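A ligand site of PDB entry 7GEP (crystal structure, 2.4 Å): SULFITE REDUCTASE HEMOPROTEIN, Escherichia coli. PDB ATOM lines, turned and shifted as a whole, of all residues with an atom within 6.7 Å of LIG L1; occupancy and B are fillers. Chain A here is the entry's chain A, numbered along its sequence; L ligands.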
ATOM      1  N   ALA A 360       9.145  17.285 -13.020  1.00  0.00           N
ATOM      2  CA  ALA A 360       7.970  17.638 -12.218  1.00  0.00           C
ATOM      3  C   ALA A 360       7.299  18.819 -12.887  1.00  0.00           C
ATOM      4  O   ALA A 360       7.906  19.498 -13.711  1.00  0.00           O
ATOM      5  CB  ALA A 360       8.357  18.033 -10.826  1.00  0.00           C
ATOM      6  N   CYS A 361       6.043  19.034 -12.563  1.00  0.00           N
ATOM      7  CA  CYS A 361       5.330  20.158 -13.128  1.00  0.00           C
ATOM      8  C   CYS A 361       5.466  21.335 -12.152  1.00  0.00           C
ATOM      9  O   CYS A 361       6.023  21.202 -11.052  1.00  0.00           O
ATOM     10  CB  CYS A 361       3.871  19.791 -13.381  1.00  0.00           C
ATOM     11  SG  CYS A 361       2.966  19.525 -11.833  1.00  0.00           S
ATOM     12  N   VAL A 362       4.947  22.489 -12.581  1.00  0.00           N
ATOM     13  CA  VAL A 362       4.983  23.700 -11.781  1.00  0.00           C
ATOM     14  C   VAL A 362       4.285  23.536 -10.433  1.00  0.00           C
ATOM     15  O   VAL A 362       4.894  23.695  -9.363  1.00  0.00           O
ATOM     16  CB  VAL A 362       4.319  24.844 -12.544  1.00  0.00           C
ATOM     17  CG1 VAL A 362       4.405  26.104 -11.736  1.00  0.00           C
ATOM     18  CG2 VAL A 362       4.974  25.021 -13.908  1.00  0.00           C
ATOM     19  N   SER A 363       3.004  23.152 -10.505  1.00  0.00           N
ATOM     20  CA  SER A 363       2.170  22.956  -9.332  1.00  0.00           C
ATOM     21  C   SER A 363       2.043  24.256  -8.536  1.00  0.00           C
ATOM     22  O   SER A 363       1.876  25.330  -9.122  1.00  0.00           O
ATOM     23  CB  SER A 363       2.706  21.850  -8.459  1.00  0.00           C
ATOM     24  OG  SER A 363       1.717  21.445  -7.553  1.00  0.00           O
ATOM     25  N   PHE A 364       2.140  24.160  -7.210  1.00  0.00           N
ATOM     26  CA  PHE A 364       2.027  25.338  -6.371  1.00  0.00           C
ATOM     27  C   PHE A 364       3.278  26.136  -6.583  1.00  0.00           C
ATOM     28  O   PHE A 364       4.319  25.549  -6.845  1.00  0.00           O
ATOM     29  CB  PHE A 364       1.919  24.958  -4.900  1.00  0.00           C
ATOM     30  CG  PHE A 364       0.679  24.201  -4.585  1.00  0.00           C
ATOM     31  CD1 PHE A 364      -0.561  24.808  -4.657  1.00  0.00           C
ATOM     32  CD2 PHE A 364       0.759  22.869  -4.177  1.00  0.00           C
ATOM     33  CE1 PHE A 364      -1.735  24.088  -4.365  1.00  0.00           C
ATOM     34  CE2 PHE A 364      -0.393  22.140  -3.883  1.00  0.00           C
ATOM     35  CZ  PHE A 364      -1.642  22.758  -3.954  1.00  0.00           C
ATOM     36  N   CYS A 367      -0.234  27.155  -9.832  1.00  0.00           N
ATOM     37  CA  CYS A 367      -1.277  26.356 -10.433  1.00  0.00           C
ATOM     38  C   CYS A 367      -2.509  26.281  -9.564  1.00  0.00           C
ATOM     39  O   CYS A 367      -2.449  25.859  -8.409  1.00  0.00           O
ATOM     40  CB  CYS A 367      -0.821  24.957 -10.809  1.00  0.00           C
ATOM     41  SG  CYS A 367      -2.062  24.088 -11.810  1.00  0.00           S
ATOM     42  N   PRO A 368      -3.650  26.667 -10.125  1.00  0.00           N
ATOM     43  CA  PRO A 368      -4.920  26.654  -9.398  1.00  0.00           C
ATOM     44  C   PRO A 368      -5.540  25.237  -9.294  1.00  0.00           C
ATOM     45  O   PRO A 368      -6.481  25.007  -8.522  1.00  0.00           O
ATOM     46  CB  PRO A 368      -5.790  27.587 -10.237  1.00  0.00           C
ATOM     47  CG  PRO A 368      -5.305  27.348 -11.628  1.00  0.00           C
ATOM     48  CD  PRO A 368      -3.807  27.292 -11.467  1.00  0.00           C
ATOM     49  N   LEU A 369      -5.004  24.289 -10.059  1.00  0.00           N
ATOM     50  CA  LEU A 369      -5.532  22.942 -10.062  1.00  0.00           C
ATOM     51  C   LEU A 369      -4.679  22.008  -9.250  1.00  0.00           C
ATOM     52  O   LEU A 369      -5.007  20.831  -9.115  1.00  0.00           O
ATOM     53  CB  LEU A 369      -5.623  22.436 -11.495  1.00  0.00           C
ATOM     54  CG  LEU A 369      -6.223  23.376 -12.537  1.00  0.00           C
ATOM     55  CD1 LEU A 369      -6.337  22.676 -13.885  1.00  0.00           C
ATOM     56  CD2 LEU A 369      -7.579  23.828 -12.064  1.00  0.00           C
ATOM     57  N   ALA A 370      -3.626  22.540  -8.645  1.00  0.00           N
ATOM     58  CA  ALA A 370      -2.690  21.759  -7.864  1.00  0.00           C
ATOM     59  C   ALA A 370      -3.278  21.076  -6.615  1.00  0.00           C
ATOM     60  O   ALA A 370      -4.124  21.656  -5.930  1.00  0.00           O
ATOM     61  CB  ALA A 370      -1.493  22.621  -7.499  1.00  0.00           C
ATOM     62  N   MET A 371      -2.838  19.847  -6.370  1.00  0.00           N
ATOM     63  CA  MET A 371      -3.265  19.068  -5.217  1.00  0.00           C
ATOM     64  C   MET A 371      -2.059  18.799  -4.313  1.00  0.00           C
ATOM     65  O   MET A 371      -2.145  18.954  -3.097  1.00  0.00           O
ATOM     66  CB  MET A 371      -3.866  17.731  -5.676  1.00  0.00           C
ATOM     67  CG  MET A 371      -5.227  17.842  -6.392  1.00  0.00           C
ATOM     68  SD  MET A 371      -5.750  16.299  -7.242  1.00  0.00           S
ATOM     69  CE  MET A 371      -7.195  16.835  -8.236  1.00  0.00           C
ATOM     70  N   ALA A 372      -0.924  18.460  -4.913  1.00  0.00           N
ATOM     71  CA  ALA A 372       0.306  18.171  -4.197  1.00  0.00           C
ATOM     72  C   ALA A 372       1.444  18.947  -4.862  1.00  0.00           C
ATOM     73  O   ALA A 372       1.359  19.271  -6.047  1.00  0.00           O
ATOM     74  CB  ALA A 372       0.604  16.684  -4.260  1.00  0.00           C
ATOM     75  N   ALA A 374       5.030  19.749  -6.621  1.00  0.00           N
ATOM     76  CA  ALA A 374       5.746  19.021  -7.668  1.00  0.00           C
ATOM     77  C   ALA A 374       7.092  19.694  -7.878  1.00  0.00           C
ATOM     78  O   ALA A 374       8.120  19.170  -7.438  1.00  0.00           O
ATOM     79  CB  ALA A 374       4.910  19.019  -8.969  1.00  0.00           C
ATOM     80  N   VAL A 403       7.053  13.622 -11.307  1.00  0.00           N
ATOM     81  CA  VAL A 403       6.036  13.962 -10.338  1.00  0.00           C
ATOM     82  C   VAL A 403       5.082  14.954 -10.964  1.00  0.00           C
ATOM     83  O   VAL A 403       5.497  15.979 -11.493  1.00  0.00           O
ATOM     84  CB  VAL A 403       6.679  14.617  -9.078  1.00  0.00           C
ATOM     85  CG1 VAL A 403       5.627  15.056  -8.101  1.00  0.00           C
ATOM     86  CG2 VAL A 403       7.631  13.624  -8.399  1.00  0.00           C
ATOM     87  N   THR A 404       3.811  14.626 -10.977  1.00  0.00           N
ATOM     88  CA  THR A 404       2.816  15.530 -11.524  1.00  0.00           C
ATOM     89  C   THR A 404       1.949  15.944 -10.330  1.00  0.00           C
ATOM     90  O   THR A 404       1.594  15.093  -9.505  1.00  0.00           O
ATOM     91  CB  THR A 404       2.043  14.846 -12.734  1.00  0.00           C
ATOM     92  OG1 THR A 404       1.311  15.839 -13.462  1.00  0.00           O
ATOM     93  CG2 THR A 404       1.115  13.738 -12.280  1.00  0.00           C
ATOM     94  N   GLY A 405       1.745  17.253 -10.154  1.00  0.00           N
ATOM     95  CA  GLY A 405       0.954  17.786  -9.050  1.00  0.00           C
ATOM     96  C   GLY A 405      -0.536  17.491  -8.926  1.00  0.00           C
ATOM     97  O   GLY A 405      -1.141  17.735  -7.892  1.00  0.00           O
ATOM     98  N   CYS A 406      -1.141  17.016 -10.006  1.00  0.00           N
ATOM     99  CA  CYS A 406      -2.543  16.647 -10.027  1.00  0.00           C
ATOM    100  C   CYS A 406      -2.609  15.669 -11.187  1.00  0.00           C
ATOM    101  O   CYS A 406      -1.645  15.559 -11.948  1.00  0.00           O
ATOM    102  CB  CYS A 406      -3.463  17.870 -10.183  1.00  0.00           C
ATOM    103  SG  CYS A 406      -3.701  18.555 -11.854  1.00  0.00           S
ATOM    104  N   PRO A 407      -3.729  14.965 -11.377  1.00  0.00           N
ATOM    105  CA  PRO A 407      -3.758  14.028 -12.491  1.00  0.00           C
ATOM    106  C   PRO A 407      -3.823  14.539 -13.938  1.00  0.00           C
ATOM    107  O   PRO A 407      -3.728  13.724 -14.866  1.00  0.00           O
ATOM    108  CB  PRO A 407      -4.927  13.108 -12.104  1.00  0.00           C
ATOM    109  CG  PRO A 407      -5.851  14.011 -11.438  1.00  0.00           C
ATOM    110  CD  PRO A 407      -4.974  14.899 -10.593  1.00  0.00           C
ATOM    111  N   ASN A 408      -3.944  15.848 -14.153  1.00  0.00           N
ATOM    112  CA  ASN A 408      -3.980  16.398 -15.507  1.00  0.00           C
ATOM    113  C   ASN A 408      -2.757  15.906 -16.283  1.00  0.00           C
ATOM    114  O   ASN A 408      -2.758  15.838 -17.515  1.00  0.00           O
ATOM    115  CB  ASN A 408      -4.060  17.932 -15.512  1.00  0.00           C
ATOM    116  CG  ASN A 408      -5.457  18.459 -15.171  1.00  0.00           C
ATOM    117  OD1 ASN A 408      -6.480  17.843 -15.503  1.00  0.00           O
ATOM    118  ND2 ASN A 408      -5.505  19.627 -14.553  1.00  0.00           N
ATOM    119  N   GLY A 409      -1.702  15.553 -15.522  1.00  0.00           N
ATOM    120  CA  GLY A 409      -0.506  14.957 -16.095  1.00  0.00           C
ATOM    121  C   GLY A 409       0.586  15.774 -16.731  1.00  0.00           C
ATOM    122  O   GLY A 409       1.421  15.198 -17.436  1.00  0.00           O
ATOM    123  N   CYS A 410       0.648  17.071 -16.425  1.00  0.00           N
ATOM    124  CA  CYS A 410       1.638  17.963 -16.998  1.00  0.00           C
ATOM    125  C   CYS A 410       3.103  17.534 -16.771  1.00  0.00           C
ATOM    126  O   CYS A 410       3.941  17.714 -17.657  1.00  0.00           O
ATOM    127  CB  CYS A 410       1.403  19.378 -16.497  1.00  0.00           C
ATOM    128  SG  CYS A 410      -0.352  19.898 -16.627  1.00  0.00           S
ATOM    129  N   GLY A 411       3.402  16.907 -15.642  1.00  0.00           N
ATOM    130  CA  GLY A 411       4.776  16.460 -15.422  1.00  0.00           C
ATOM    131  C   GLY A 411       5.124  15.177 -16.172  1.00  0.00           C
ATOM    132  O   GLY A 411       6.232  14.646 -16.029  1.00  0.00           O
HETATM  133 FE1  LIG L   1       0.808  20.157 -12.235  1.00  0.00          FE
HETATM  134 FE2  LIG L   1      -0.976  22.196 -12.437  1.00  0.00          FE
HETATM  135 FE3  LIG L   1      -1.828  19.630 -12.303  1.00  0.00          FE
HETATM  136 FE4  LIG L   1      -0.536  20.494 -14.502  1.00  0.00          FE
HETATM  137  S1  LIG L   1      -2.552  21.276 -13.778  1.00  0.00           S
HETATM  138  S2  LIG L   1      -0.238  18.483 -13.415  1.00  0.00           S
HETATM  139  S3  LIG L   1       1.002  21.997 -13.589  1.00  0.00           S
HETATM  140  S4  LIG L   1      -0.646  20.792 -10.691  1.00  0.00           S
HETATM  141 FE1  LG2 L   2      -0.534  21.456 -18.490  1.00  0.00          FE
HETATM  142  C1  LG2 L   2      -3.360  22.723 -17.324  1.00  0.00           C
HETATM  143  C2  LG2 L   2       1.302  23.695 -16.757  1.00  0.00           C
HETATM  144  C3  LG2 L   2       2.284  20.434 -20.180  1.00  0.00           C
HETATM  145  C4  LG2 L   2      -2.070  18.543 -19.294  1.00  0.00           C
HETATM  146  N1  LG2 L   2      -0.935  23.011 -17.291  1.00  0.00           N
HETATM  147  C5  LG2 L   2      -2.203  23.439 -16.998  1.00  0.00           C
HETATM  148  C6  LG2 L   2      -2.104  24.819 -16.404  1.00  0.00           C
HETATM  149  C7  LG2 L   2      -2.020  25.825 -17.571  1.00  0.00           C
HETATM  150  C8  LG2 L   2      -3.136  25.096 -15.320  1.00  0.00           C
HETATM  151  C9  LG2 L   2      -4.437  25.741 -15.701  1.00  0.00           C
HETATM  152  O1  LG2 L   2      -5.201  25.166 -16.500  1.00  0.00           O
HETATM  153  O2  LG2 L   2      -4.725  26.837 -15.183  1.00  0.00           O
HETATM  154  C10 LG2 L   2      -0.826  24.699 -15.703  1.00  0.00           C
HETATM  155  C11 LG2 L   2      -0.201  25.976 -15.480  1.00  0.00           C
HETATM  156  C12 LG2 L   2       0.342  26.065 -14.064  1.00  0.00           C
HETATM  157  C13 LG2 L   2       1.454  27.073 -13.947  1.00  0.00           C
HETATM  158  O3  LG2 L   2       1.353  27.978 -13.117  1.00  0.00           O
HETATM  159  O4  LG2 L   2       2.431  26.984 -14.712  1.00  0.00           O
HETATM  160  C14 LG2 L   2      -0.045  23.744 -16.569  1.00  0.00           C
HETATM  161  N2  LG2 L   2       1.416  22.060 -18.561  1.00  0.00           N
HETATM  162  C15 LG2 L   2       1.996  22.960 -17.682  1.00  0.00           C
HETATM  163  C16 LG2 L   2       3.508  22.866 -17.837  1.00  0.00           C
HETATM  164  C17 LG2 L   2       4.185  24.275 -17.667  1.00  0.00           C
HETATM  165  C18 LG2 L   2       4.157  21.825 -16.838  1.00  0.00           C
HETATM  166  C19 LG2 L   2       5.663  21.974 -16.652  1.00  0.00           C
HETATM  167  O5  LG2 L   2       6.131  22.028 -15.505  1.00  0.00           O
HETATM  168  O6  LG2 L   2       6.395  22.055 -17.642  1.00  0.00           O
HETATM  169  C20 LG2 L   2       3.555  22.447 -19.364  1.00  0.00           C
HETATM  170  C21 LG2 L   2       3.367  23.609 -20.268  1.00  0.00           C
HETATM  171  C22 LG2 L   2       3.174  23.128 -21.682  1.00  0.00           C
HETATM  172  C23 LG2 L   2       3.302  24.240 -22.693  1.00  0.00           C
HETATM  173  O7  LG2 L   2       4.173  25.101 -22.514  1.00  0.00           O
HETATM  174  O8  LG2 L   2       2.542  24.230 -23.670  1.00  0.00           O
HETATM  175  C24 LG2 L   2       2.371  21.553 -19.403  1.00  0.00           C
HETATM  176  N3  LG2 L   2       0.035  19.818 -19.563  1.00  0.00           N
HETATM  177  C25 LG2 L   2       1.191  19.626 -20.254  1.00  0.00           C
HETATM  178  C26 LG2 L   2       1.298  18.143 -20.533  1.00  0.00           C
HETATM  179  C27 LG2 L   2       2.559  17.444 -20.965  1.00  0.00           C
HETATM  180  C28 LG2 L   2       2.931  17.641 -22.412  1.00  0.00           C
HETATM  181  O9  LG2 L   2       2.120  18.227 -23.157  1.00  0.00           O
HETATM  182  O10 LG2 L   2       4.029  17.218 -22.810  1.00  0.00           O
HETATM  183  C29 LG2 L   2       0.112  17.563 -20.267  1.00  0.00           C
HETATM  184  C30 LG2 L   2      -0.150  16.086 -20.218  1.00  0.00           C
HETATM  185  C31 LG2 L   2      -0.398  15.478 -21.564  1.00  0.00           C
HETATM  186  C32 LG2 L   2      -1.781  15.753 -22.078  1.00  0.00           C
HETATM  187  O11 LG2 L   2      -2.032  16.879 -22.526  1.00  0.00           O
HETATM  188  O12 LG2 L   2      -2.620  14.836 -22.049  1.00  0.00           O
HETATM  189  C33 LG2 L   2      -0.743  18.657 -19.666  1.00  0.00           C
HETATM  190  N4  LG2 L   2      -2.430  20.782 -18.466  1.00  0.00           N
HETATM  191  C34 LG2 L   2      -2.877  19.516 -18.790  1.00  0.00           C
HETATM  192  C35 LG2 L   2      -4.336  19.399 -18.519  1.00  0.00           C
HETATM  193  C36 LG2 L   2      -5.162  18.150 -18.731  1.00  0.00           C
HETATM  194  C37 LG2 L   2      -5.826  18.392 -20.062  1.00  0.00           C
HETATM  195  C38 LG2 L   2      -6.705  17.259 -20.518  1.00  0.00           C
HETATM  196  O13 LG2 L   2      -6.740  17.015 -21.729  1.00  0.00           O
HETATM  197  O14 LG2 L   2      -7.342  16.608 -19.674  1.00  0.00           O
HETATM  198  C39 LG2 L   2      -4.684  20.650 -18.013  1.00  0.00           C
HETATM  199  C40 LG2 L   2      -5.981  21.213 -17.538  1.00  0.00           C
HETATM  200  C41 LG2 L   2      -6.969  21.414 -18.666  1.00  0.00           C
HETATM  201  O15 LG2 L   2      -6.541  21.680 -19.808  1.00  0.00           O
HETATM  202  O16 LG2 L   2      -8.173  21.285 -18.399  1.00  0.00           O
HETATM  203  C42 LG2 L   2      -3.465  21.510 -17.984  1.00  0.00           C
HETATM  204  S1  LG3 L   3      -0.571  22.588 -20.387  1.00  0.00           S
HETATM  205  O1  LG3 L   3      -1.183  22.200 -21.898  1.00  0.00           O
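The backbone NH (N) of Cys 410 lies close to a sulfur (S2) of LIG L1 (3.4 Å). A sulfur (S1) of LIG L1 lies close to the side-chain amide nitrogen (ND2) of Asn 408, 3.5 Å away. SG of Cys 406 binds FE3 of LIG L1. The backbone NH (N) of Val 362 lies within hydrogen-bond range of an oxygen (O5) of LG2 L2, at 3.2 Å. S2 of LIG L1 lies close to OG1 of Thr 404, at 3.1 Å. The side-chain sulfur of Cys 410 binds an iron atom (FE4) of LIG L1, at 2.2 Å. The side-chain sulfur (SG) of Cys 410 is bound to an iron atom (FE1) of LG2 L2 (2.4 Å). An iron atom (FE1) of LIG L1 is bound by the side-chain sulfur (SG) of Cys 361 (2.3 Å). SG of Cys 367 binds FE2 of LIG L1 (2.3 Å).
S1 of LG3 L3 binds FE1 of LG2 L2 (2.2 Å).
The side-chain sulfur (SG) of Cys 406 sits close to the side-chain amide nitrogen (ND2) of Asn 408. O of Gly 405 sits at hydrogen-bond distance from N of Ala 372 (3.1 Å). The backbone NH of Cys 410 lies within hydrogen-bond range of the side-chain hydroxyl of Thr 404 (3.3 Å). The backbone carbonyl oxygen (O) of Leu 369 lies close to the side-chain sulfur (SG) of Cys 406 (3.8 Å). The backbone NH (N) of Cys 361 is in hydrogen-bond range of the backbone carbonyl oxygen (O) of Val 403 (3.3 Å). The backbone carbonyl oxygen (O) of Cys 406 lies close to the side-chain hydroxyl (OG1) of Thr 404 (3.3 Å). The backbone NH (N) of Met 371 lies within hydrogen-bond range of the backbone carbonyl oxygen (O) of Gly 405 (3.1 Å). The side-chain sulfur of Cys 367 sits close to the backbone NH of Leu 369, 3.4 Å away.
Residues that only touch LIG L1: Ser 363 (3.8 Å), Leu 369 (3.999 Å), Ala 370 (3.6 Å), Gly 405 (3.7 Å) and Gly 409 (3.9 Å). Hydrophobic or aromatic side chains within 4 Å of LIG L1: Leu 369 and Ala 370. Within 4 Å of LIG L1: Cys 361, Ser 363, Cys 367, Leu 369, Ala 370, Thr 404, Gly 405, Cys 406, Asn 408, Gly 409 and Cys 410. The nearest printed residue that does not touch LIG L1 is Val 362 (4.1 Å).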
